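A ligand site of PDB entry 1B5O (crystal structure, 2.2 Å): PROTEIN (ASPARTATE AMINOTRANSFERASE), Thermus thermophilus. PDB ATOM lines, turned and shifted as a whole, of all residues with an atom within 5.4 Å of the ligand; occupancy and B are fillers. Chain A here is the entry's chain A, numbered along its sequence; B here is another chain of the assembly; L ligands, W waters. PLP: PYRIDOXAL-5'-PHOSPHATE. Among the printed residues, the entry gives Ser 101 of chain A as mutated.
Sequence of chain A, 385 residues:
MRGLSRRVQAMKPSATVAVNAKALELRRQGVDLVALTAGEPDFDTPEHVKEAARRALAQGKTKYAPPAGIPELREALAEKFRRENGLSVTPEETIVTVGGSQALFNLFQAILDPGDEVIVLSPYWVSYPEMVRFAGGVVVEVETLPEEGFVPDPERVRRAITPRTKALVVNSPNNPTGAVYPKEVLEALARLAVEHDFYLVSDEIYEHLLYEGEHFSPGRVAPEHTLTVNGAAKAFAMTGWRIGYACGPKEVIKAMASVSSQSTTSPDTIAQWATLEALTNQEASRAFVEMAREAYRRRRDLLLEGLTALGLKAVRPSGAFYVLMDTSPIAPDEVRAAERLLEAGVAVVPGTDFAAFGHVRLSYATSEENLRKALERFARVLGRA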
ATOM      1  N   GLY A  39      -4.194  -2.788  18.930  1.00  0.00           N
ATOM      2  CA  GLY A  39      -4.824  -1.692  19.672  1.00  0.00           C
ATOM      3  C   GLY A  39      -5.233  -0.598  18.705  1.00  0.00           C
ATOM      4  O   GLY A  39      -5.505   0.534  19.110  1.00  0.00           O
ATOM      5  N   VAL A  98      -1.062  16.007  19.847  1.00  0.00           N
ATOM      6  CA  VAL A  98      -0.385  14.937  19.111  1.00  0.00           C
ATOM      7  C   VAL A  98      -0.946  13.635  19.692  1.00  0.00           C
ATOM      8  O   VAL A  98      -0.366  13.032  20.600  1.00  0.00           O
ATOM      9  CB  VAL A  98       1.158  14.998  19.279  1.00  0.00           C
ATOM     10  CG1 VAL A  98       1.824  13.881  18.488  1.00  0.00           C
ATOM     11  CG2 VAL A  98       1.684  16.350  18.815  1.00  0.00           C
ATOM     12  N   GLY A  99      -2.118  13.251  19.191  1.00  0.00           N
ATOM     13  CA  GLY A  99      -2.784  12.061  19.671  1.00  0.00           C
ATOM     14  C   GLY A  99      -3.550  12.328  20.949  1.00  0.00           C
ATOM     15  O   GLY A  99      -3.303  13.325  21.659  1.00  0.00           O
ATOM     16  N   GLY A 100      -4.520  11.476  21.233  1.00  0.00           N
ATOM     17  CA  GLY A 100      -5.302  11.618  22.450  1.00  0.00           C
ATOM     18  C   GLY A 100      -4.384  11.393  23.634  1.00  0.00           C
ATOM     19  O   GLY A 100      -4.653  11.861  24.740  1.00  0.00           O
ATOM     20  N   SER A 101      -3.269  10.698  23.407  1.00  0.00           N
ATOM     21  CA  SER A 101      -2.323  10.421  24.480  1.00  0.00           C
ATOM     22  C   SER A 101      -1.655  11.714  24.973  1.00  0.00           C
ATOM     23  O   SER A 101      -1.408  11.860  26.170  1.00  0.00           O
ATOM     24  CB  SER A 101      -1.279   9.394  24.058  1.00  0.00           C
ATOM     25  OG  SER A 101      -0.475   9.879  22.990  1.00  0.00           O
ATOM     26  N   GLN A 102      -1.397  12.653  24.064  1.00  0.00           N
ATOM     27  CA  GLN A 102      -0.751  13.908  24.471  1.00  0.00           C
ATOM     28  C   GLN A 102      -1.725  14.793  25.220  1.00  0.00           C
ATOM     29  O   GLN A 102      -1.322  15.545  26.101  1.00  0.00           O
ATOM     30  CB  GLN A 102      -0.157  14.683  23.285  1.00  0.00           C
ATOM     31  CG  GLN A 102       0.949  15.616  23.757  1.00  0.00           C
ATOM     32  CD  GLN A 102       1.157  16.835  22.885  1.00  0.00           C
ATOM     33  OE1 GLN A 102       0.347  17.152  22.024  1.00  0.00           O
ATOM     34  NE2 GLN A 102       2.248  17.536  23.122  1.00  0.00           N
ATOM     35  N   LEU A 104      -3.981  13.825  27.291  1.00  0.00           N
ATOM     36  CA  LEU A 104      -3.956  13.304  28.649  1.00  0.00           C
ATOM     37  C   LEU A 104      -2.664  13.668  29.350  1.00  0.00           C
ATOM     38  O   LEU A 104      -2.687  14.044  30.517  1.00  0.00           O
ATOM     39  CB  LEU A 104      -4.119  11.779  28.618  1.00  0.00           C
ATOM     40  CG  LEU A 104      -5.525  11.282  28.343  1.00  0.00           C
ATOM     41  CD1 LEU A 104      -5.483   9.868  27.771  1.00  0.00           C
ATOM     42  CD2 LEU A 104      -6.346  11.348  29.633  1.00  0.00           C
ATOM     43  N   TRP A 125      -6.561   1.406  31.164  1.00  0.00           N
ATOM     44  CA  TRP A 125      -5.647   1.487  30.037  1.00  0.00           C
ATOM     45  C   TRP A 125      -4.253   1.692  30.650  1.00  0.00           C
ATOM     46  O   TRP A 125      -4.071   2.507  31.549  1.00  0.00           O
ATOM     47  CB  TRP A 125      -6.033   2.674  29.164  1.00  0.00           C
ATOM     48  CG  TRP A 125      -5.251   2.824  27.915  1.00  0.00           C
ATOM     49  CD1 TRP A 125      -4.875   1.835  27.053  1.00  0.00           C
ATOM     50  CD2 TRP A 125      -4.773   4.058  27.346  1.00  0.00           C
ATOM     51  NE1 TRP A 125      -4.207   2.367  25.975  1.00  0.00           N
ATOM     52  CE2 TRP A 125      -4.130   3.728  26.135  1.00  0.00           C
ATOM     53  CE3 TRP A 125      -4.838   5.395  27.743  1.00  0.00           C
ATOM     54  CZ2 TRP A 125      -3.562   4.707  25.310  1.00  0.00           C
ATOM     55  CZ3 TRP A 125      -4.272   6.367  26.931  1.00  0.00           C
ATOM     56  CH2 TRP A 125      -3.641   6.010  25.726  1.00  0.00           C
ATOM     57  N   TYR A 128      -2.652   5.368  31.870  1.00  0.00           N
ATOM     58  CA  TYR A 128      -3.147   6.241  32.942  1.00  0.00           C
ATOM     59  C   TYR A 128      -2.223   6.324  34.163  1.00  0.00           C
ATOM     60  O   TYR A 128      -1.786   7.421  34.523  1.00  0.00           O
ATOM     61  CB  TYR A 128      -4.559   5.821  33.380  1.00  0.00           C
ATOM     62  CG  TYR A 128      -5.640   5.990  32.336  1.00  0.00           C
ATOM     63  CD1 TYR A 128      -5.496   6.873  31.274  1.00  0.00           C
ATOM     64  CD2 TYR A 128      -6.817   5.240  32.421  1.00  0.00           C
ATOM     65  CE1 TYR A 128      -6.502   7.001  30.300  1.00  0.00           C
ATOM     66  CE2 TYR A 128      -7.818   5.364  31.471  1.00  0.00           C
ATOM     67  CZ  TYR A 128      -7.663   6.238  30.423  1.00  0.00           C
ATOM     68  OH  TYR A 128      -8.651   6.306  29.465  1.00  0.00           O
ATOM     69  N   ASN A 171     -13.359   6.128  31.474  1.00  0.00           N
ATOM     70  CA  ASN A 171     -13.140   5.722  30.088  1.00  0.00           C
ATOM     71  C   ASN A 171     -14.291   4.853  29.581  1.00  0.00           C
ATOM     72  O   ASN A 171     -14.377   3.676  29.907  1.00  0.00           O
ATOM     73  CB  ASN A 171     -11.792   4.985  30.016  1.00  0.00           C
ATOM     74  CG  ASN A 171     -11.459   4.439  28.623  1.00  0.00           C
ATOM     75  OD1 ASN A 171     -10.850   3.375  28.498  1.00  0.00           O
ATOM     76  ND2 ASN A 171     -11.804   5.194  27.578  1.00  0.00           N
ATOM     77  N   ASN A 175     -11.417   0.407  27.402  1.00  0.00           N
ATOM     78  CA  ASN A 175     -10.287  -0.380  26.921  1.00  0.00           C
ATOM     79  C   ASN A 175      -9.650  -0.726  28.278  1.00  0.00           C
ATOM     80  O   ASN A 175      -9.248   0.179  29.009  1.00  0.00           O
ATOM     81  CB  ASN A 175      -9.347   0.494  26.078  1.00  0.00           C
ATOM     82  CG  ASN A 175      -8.054  -0.233  25.677  1.00  0.00           C
ATOM     83  OD1 ASN A 175      -7.794  -1.355  26.111  1.00  0.00           O
ATOM     84  ND2 ASN A 175      -7.230   0.434  24.865  1.00  0.00           N
ATOM     85  N   ASP A 203     -12.311  10.062  28.994  1.00  0.00           N
ATOM     86  CA  ASP A 203     -11.649   9.580  27.777  1.00  0.00           C
ATOM     87  C   ASP A 203     -12.732   8.931  26.905  1.00  0.00           C
ATOM     88  O   ASP A 203     -13.136   7.803  27.157  1.00  0.00           O
ATOM     89  CB  ASP A 203     -10.554   8.567  28.139  1.00  0.00           C
ATOM     90  CG  ASP A 203      -9.623   8.257  26.971  1.00  0.00           C
ATOM     91  OD1 ASP A 203      -9.937   8.590  25.818  1.00  0.00           O
ATOM     92  OD2 ASP A 203      -8.541   7.692  27.226  1.00  0.00           O
ATOM     93  N   ILE A 205     -12.559   8.372  23.325  1.00  0.00           N
ATOM     94  CA  ILE A 205     -12.100   7.999  21.973  1.00  0.00           C
ATOM     95  C   ILE A 205     -12.867   6.891  21.260  1.00  0.00           C
ATOM     96  O   ILE A 205     -12.836   6.846  20.036  1.00  0.00           O
ATOM     97  CB  ILE A 205     -10.603   7.597  21.903  1.00  0.00           C
ATOM     98  CG1 ILE A 205     -10.071   7.182  23.259  1.00  0.00           C
ATOM     99  CG2 ILE A 205      -9.761   8.712  21.281  1.00  0.00           C
ATOM    100  CD1 ILE A 205     -10.686   5.933  23.804  1.00  0.00           C
ATOM    101  N   TYR A 206     -13.490   5.974  21.996  1.00  0.00           N
ATOM    102  CA  TYR A 206     -14.256   4.877  21.398  1.00  0.00           C
ATOM    103  C   TYR A 206     -15.742   5.154  21.210  1.00  0.00           C
ATOM    104  O   TYR A 206     -16.502   4.242  20.883  1.00  0.00           O
ATOM    105  CB  TYR A 206     -14.105   3.590  22.213  1.00  0.00           C
ATOM    106  CG  TYR A 206     -12.744   2.961  22.117  1.00  0.00           C
ATOM    107  CD1 TYR A 206     -12.352   2.299  20.955  1.00  0.00           C
ATOM    108  CD2 TYR A 206     -11.835   3.061  23.162  1.00  0.00           C
ATOM    109  CE1 TYR A 206     -11.078   1.750  20.842  1.00  0.00           C
ATOM    110  CE2 TYR A 206     -10.564   2.534  23.054  1.00  0.00           C
ATOM    111  CZ  TYR A 206     -10.193   1.880  21.902  1.00  0.00           C
ATOM    112  OH  TYR A 206      -8.920   1.368  21.787  1.00  0.00           O
ATOM    113  N   GLY A 231     -10.330  11.983  19.993  1.00  0.00           N
ATOM    114  CA  GLY A 231      -9.359  11.946  18.913  1.00  0.00           C
ATOM    115  C   GLY A 231      -9.851  11.212  17.679  1.00  0.00           C
ATOM    116  O   GLY A 231     -10.859  10.514  17.724  1.00  0.00           O
ATOM    117  N   ALA A 233      -7.983   8.900  16.039  1.00  0.00           N
ATOM    118  CA  ALA A 233      -7.326   7.588  15.980  1.00  0.00           C
ATOM    119  C   ALA A 233      -8.162   6.337  15.737  1.00  0.00           C
ATOM    120  O   ALA A 233      -7.984   5.662  14.732  1.00  0.00           O
ATOM    121  CB  ALA A 233      -6.441   7.391  17.201  1.00  0.00           C
ATOM    122  N   LYS A 234      -9.058   6.026  16.677  1.00  0.00           N
ATOM    123  CA  LYS A 234      -9.861   4.816  16.589  1.00  0.00           C
ATOM    124  C   LYS A 234     -11.074   4.850  15.674  1.00  0.00           C
ATOM    125  O   LYS A 234     -11.383   3.843  15.030  1.00  0.00           O
ATOM    126  CB  LYS A 234     -10.274   4.356  17.994  1.00  0.00           C
ATOM    127  CG  LYS A 234      -9.123   4.385  19.012  1.00  0.00           C
ATOM    128  CD  LYS A 234      -8.088   3.287  18.762  1.00  0.00           C
ATOM    129  CE  LYS A 234      -6.768   3.546  19.529  1.00  0.00           C
ATOM    130  NZ  LYS A 234      -7.101   4.136  20.832  1.00  0.00           N
ATOM    131  N   THR A 239      -4.581   6.249  13.597  1.00  0.00           N
ATOM    132  CA  THR A 239      -3.627   6.112  14.691  1.00  0.00           C
ATOM    133  C   THR A 239      -2.206   6.629  14.362  1.00  0.00           C
ATOM    134  O   THR A 239      -1.521   7.166  15.226  1.00  0.00           O
ATOM    135  CB  THR A 239      -3.528   4.640  15.186  1.00  0.00           C
ATOM    136  OG1 THR A 239      -3.135   3.795  14.089  1.00  0.00           O
ATOM    137  CG2 THR A 239      -4.858   4.164  15.754  1.00  0.00           C
ATOM    138  N   ARG A 242      -1.358  10.798  14.411  1.00  0.00           N
ATOM    139  CA  ARG A 242      -1.103  11.470  15.694  1.00  0.00           C
ATOM    140  C   ARG A 242      -1.875  12.799  15.903  1.00  0.00           C
ATOM    141  O   ARG A 242      -1.263  13.865  16.048  1.00  0.00           O
ATOM    142  CB  ARG A 242       0.392  11.655  15.920  1.00  0.00           C
ATOM    143  CG  ARG A 242       1.278  10.397  15.690  1.00  0.00           C
ATOM    144  CD  ARG A 242       0.828   9.165  16.498  1.00  0.00           C
ATOM    145  NE  ARG A 242       0.756   9.396  17.944  1.00  0.00           N
ATOM    146  CZ  ARG A 242      -0.316   9.160  18.684  1.00  0.00           C
ATOM    147  NH1 ARG A 242      -1.417   8.661  18.125  1.00  0.00           N
ATOM    148  NH2 ARG A 242      -0.329   9.468  19.978  1.00  0.00           N
ATOM    149  N   ILE A 243      -3.195  12.724  15.922  1.00  0.00           N
ATOM    150  CA  ILE A 243      -4.057  13.897  16.130  1.00  0.00           C
ATOM    151  C   ILE A 243      -5.173  13.585  17.134  1.00  0.00           C
ATOM    152  O   ILE A 243      -6.030  12.737  16.896  1.00  0.00           O
ATOM    153  CB  ILE A 243      -4.700  14.396  14.815  1.00  0.00           C
ATOM    154  CG1 ILE A 243      -3.643  14.978  13.864  1.00  0.00           C
ATOM    155  CG2 ILE A 243      -5.784  15.434  15.113  1.00  0.00           C
ATOM    156  CD1 ILE A 243      -3.002  16.275  14.338  1.00  0.00           C
ATOM    157  N   GLY A 244      -5.136  14.269  18.271  1.00  0.00           N
ATOM    158  CA  GLY A 244      -6.157  14.099  19.276  1.00  0.00           C
ATOM    159  C   GLY A 244      -6.728  15.449  19.656  1.00  0.00           C
ATOM    160  O   GLY A 244      -6.254  16.477  19.171  1.00  0.00           O
ATOM    161  N   TYR A 322     -12.367  -4.996  22.025  1.00  0.00           N
ATOM    162  CA  TYR A 322     -11.661  -5.876  22.953  1.00  0.00           C
ATOM    163  C   TYR A 322     -12.620  -6.782  23.699  1.00  0.00           C
ATOM    164  O   TYR A 322     -13.825  -6.529  23.760  1.00  0.00           O
ATOM    165  CB  TYR A 322     -10.884  -5.062  23.983  1.00  0.00           C
ATOM    166  CG  TYR A 322      -9.970  -4.035  23.353  1.00  0.00           C
ATOM    167  CD1 TYR A 322      -8.851  -4.433  22.613  1.00  0.00           C
ATOM    168  CD2 TYR A 322     -10.241  -2.672  23.465  1.00  0.00           C
ATOM    169  CE1 TYR A 322      -8.032  -3.492  22.008  1.00  0.00           C
ATOM    170  CE2 TYR A 322      -9.434  -1.720  22.864  1.00  0.00           C
ATOM    171  CZ  TYR A 322      -8.322  -2.150  22.137  1.00  0.00           C
ATOM    172  OH  TYR A 322      -7.505  -1.215  21.544  1.00  0.00           O
ATOM    173  N   TYR B  64       0.445   2.922  13.928  1.00  0.00           N
ATOM    174  CA  TYR B  64       1.394   3.310  14.979  1.00  0.00           C
ATOM    175  C   TYR B  64       2.808   2.859  14.624  1.00  0.00           C
ATOM    176  O   TYR B  64       3.020   1.783  14.067  1.00  0.00           O
ATOM    177  CB  TYR B  64       1.020   2.669  16.324  1.00  0.00           C
ATOM    178  CG  TYR B  64      -0.157   3.272  17.053  1.00  0.00           C
ATOM    179  CD1 TYR B  64      -0.189   4.644  17.368  1.00  0.00           C
ATOM    180  CD2 TYR B  64      -1.202   2.466  17.486  1.00  0.00           C
ATOM    181  CE1 TYR B  64      -1.248   5.186  18.113  1.00  0.00           C
ATOM    182  CE2 TYR B  64      -2.255   2.995  18.232  1.00  0.00           C
ATOM    183  CZ  TYR B  64      -2.271   4.334  18.539  1.00  0.00           C
ATOM    184  OH  TYR B  64      -3.316   4.783  19.280  1.00  0.00           O
ATOM    185  N   THR B 265       3.532   8.947  22.080  1.00  0.00           N
ATOM    186  CA  THR B 265       3.570   7.575  21.574  1.00  0.00           C
ATOM    187  C   THR B 265       4.668   7.451  20.513  1.00  0.00           C
ATOM    188  O   THR B 265       5.644   6.743  20.714  1.00  0.00           O
ATOM    189  CB  THR B 265       2.217   7.109  20.993  1.00  0.00           C
ATOM    190  OG1 THR B 265       1.215   7.189  22.011  1.00  0.00           O
ATOM    191  CG2 THR B 265       2.311   5.654  20.513  1.00  0.00           C
HETATM  192  N1  PLP L   1      -7.426   6.217  25.383  1.00  0.00           N
HETATM  193  C2  PLP L   1      -7.671   4.917  25.082  1.00  0.00           C
HETATM  194  C2A PLP L   1      -8.405   4.043  26.093  1.00  0.00           C
HETATM  195  C3  PLP L   1      -7.259   4.412  23.894  1.00  0.00           C
HETATM  196  O3  PLP L   1      -7.495   3.114  23.588  1.00  0.00           O
HETATM  197  C4  PLP L   1      -6.580   5.242  22.981  1.00  0.00           C
HETATM  198  C4A PLP L   1      -6.140   4.637  21.662  1.00  0.00           C
HETATM  199  C5  PLP L   1      -6.346   6.588  23.324  1.00  0.00           C
HETATM  200  C6  PLP L   1      -6.774   7.042  24.522  1.00  0.00           C
HETATM  201  C5A PLP L   1      -5.610   7.610  22.454  1.00  0.00           C
HETATM  202  O4P PLP L   1      -4.843   7.236  21.328  1.00  0.00           O
HETATM  203  P   PLP L   1      -4.065   8.286  20.423  1.00  0.00           P
HETATM  204  O1P PLP L   1      -5.093   9.184  19.853  1.00  0.00           O
HETATM  205  O2P PLP L   1      -3.448   7.331  19.363  1.00  0.00           O
HETATM  206  O3P PLP L   1      -2.966   8.902  21.194  1.00  0.00           O
HETATM  207  O   HOH W   1      -6.507  10.275  18.216  1.00  0.00           O
HETATM  208  O   HOH W   2      -1.546   6.423  21.675  1.00  0.00           O
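The side-chain carboxylate (OD2) of Asp 203 lies within hydrogen-bond range of a nitrogen (N1) of the ligand (2.6 Å). The side-chain hydroxyl (OH) of Tyr 64 of chain B sits at hydrogen-bond distance from an oxygen (O2P) of the ligand (2.6 Å). The side-chain hydroxyl (OH) of Tyr 206 is in hydrogen-bond range of an oxygen (O3) of the ligand. N of Ser 101 lies within hydrogen-bond range of O3P of the ligand, at 2.9 Å. An oxygen (O3) of the ligand lies within hydrogen-bond range of the side-chain amide nitrogen (ND2) of Asn 175, 3.0 Å away. An oxygen (O1P) of the ligand lies within hydrogen-bond range of the backbone NH of Gly 100, at 2.7 Å. A carbon (C4A) of the ligand is bonded to the side-chain amino group (NZ) of Lys 234 (1.4 Å). NH1 of Arg 242 is in salt-bridge range of O2P of the ligand (2.7 Å). The side-chain hydroxyl (OG) of Ser 101 sits at hydrogen-bond distance from an oxygen (O3P) of the ligand (3.2 Å).
OH of Tyr 206 is in hydrogen-bond range of OH of Tyr 322, 3.0 Å away. NH2 of Arg 242 sits at hydrogen-bond distance from OG of Ser 101. NH2 of Arg 242 sits at hydrogen-bond distance from OG1 of Thr 265 of chain B, at 3.4 Å. The backbone carbonyl oxygen (O) of Asp 203 is in hydrogen-bond range of the side-chain amide nitrogen (ND2) of Asn 171, at 3.0 Å. The backbone carbonyl oxygen of Arg 242 sits at hydrogen-bond distance from the backbone NH of Gly 99 (3.3 Å). The side-chain hydroxyl of Tyr 206 is in hydrogen-bond range of the side-chain amino group of Lys 234 (3.4 Å). OD2 of Asp 203 lies within hydrogen-bond range of OH of Tyr 128 (2.6 Å). The backbone NH (N) of Asn 175 lies within hydrogen-bond range of the side-chain amide oxygen (OD1) of Asn 171 (3.2 Å).
Water W1 lies within hydrogen-bond range of an oxygen (O1P) of the ligand, the backbone carbonyl oxygen (O) of Ile 243 and the backbone NH (N) of Ala 233. Water W2 lies within hydrogen-bond range of the side-chain hydroxyl of Thr 265 of chain B (2.9 Å), an oxygen (O3P) of the ligand (2.9 Å) and the side-chain hydroxyl of Tyr 64 of chain B (3.4 Å).
Gly 99 touches the ligand. Trp 125 touches the ligand. Asn 171 touches the ligand. Ile 205 touches the ligand (CD1 to C2, 3.4 Å). CB of Ala 233 touches O1P of the ligand, at 3.5 Å. Hydrophobic or aromatic side chains that line the ligand: Trp 125, Ile 205, Tyr 206, Ala 233 and Tyr 64 of chain B. 13 residues have an atom within 4 Å of the ligand: Gly 99, Gly 100, Ser 101, Trp 125, Asn 171, Asn 175, Asp 203, Ile 205, Tyr 206, Ala 233, Lys 234, Arg 242 and Tyr 64 of chain B. The nearest printed residue that does not touch the ligand is Tyr 128 (4.1 Å).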
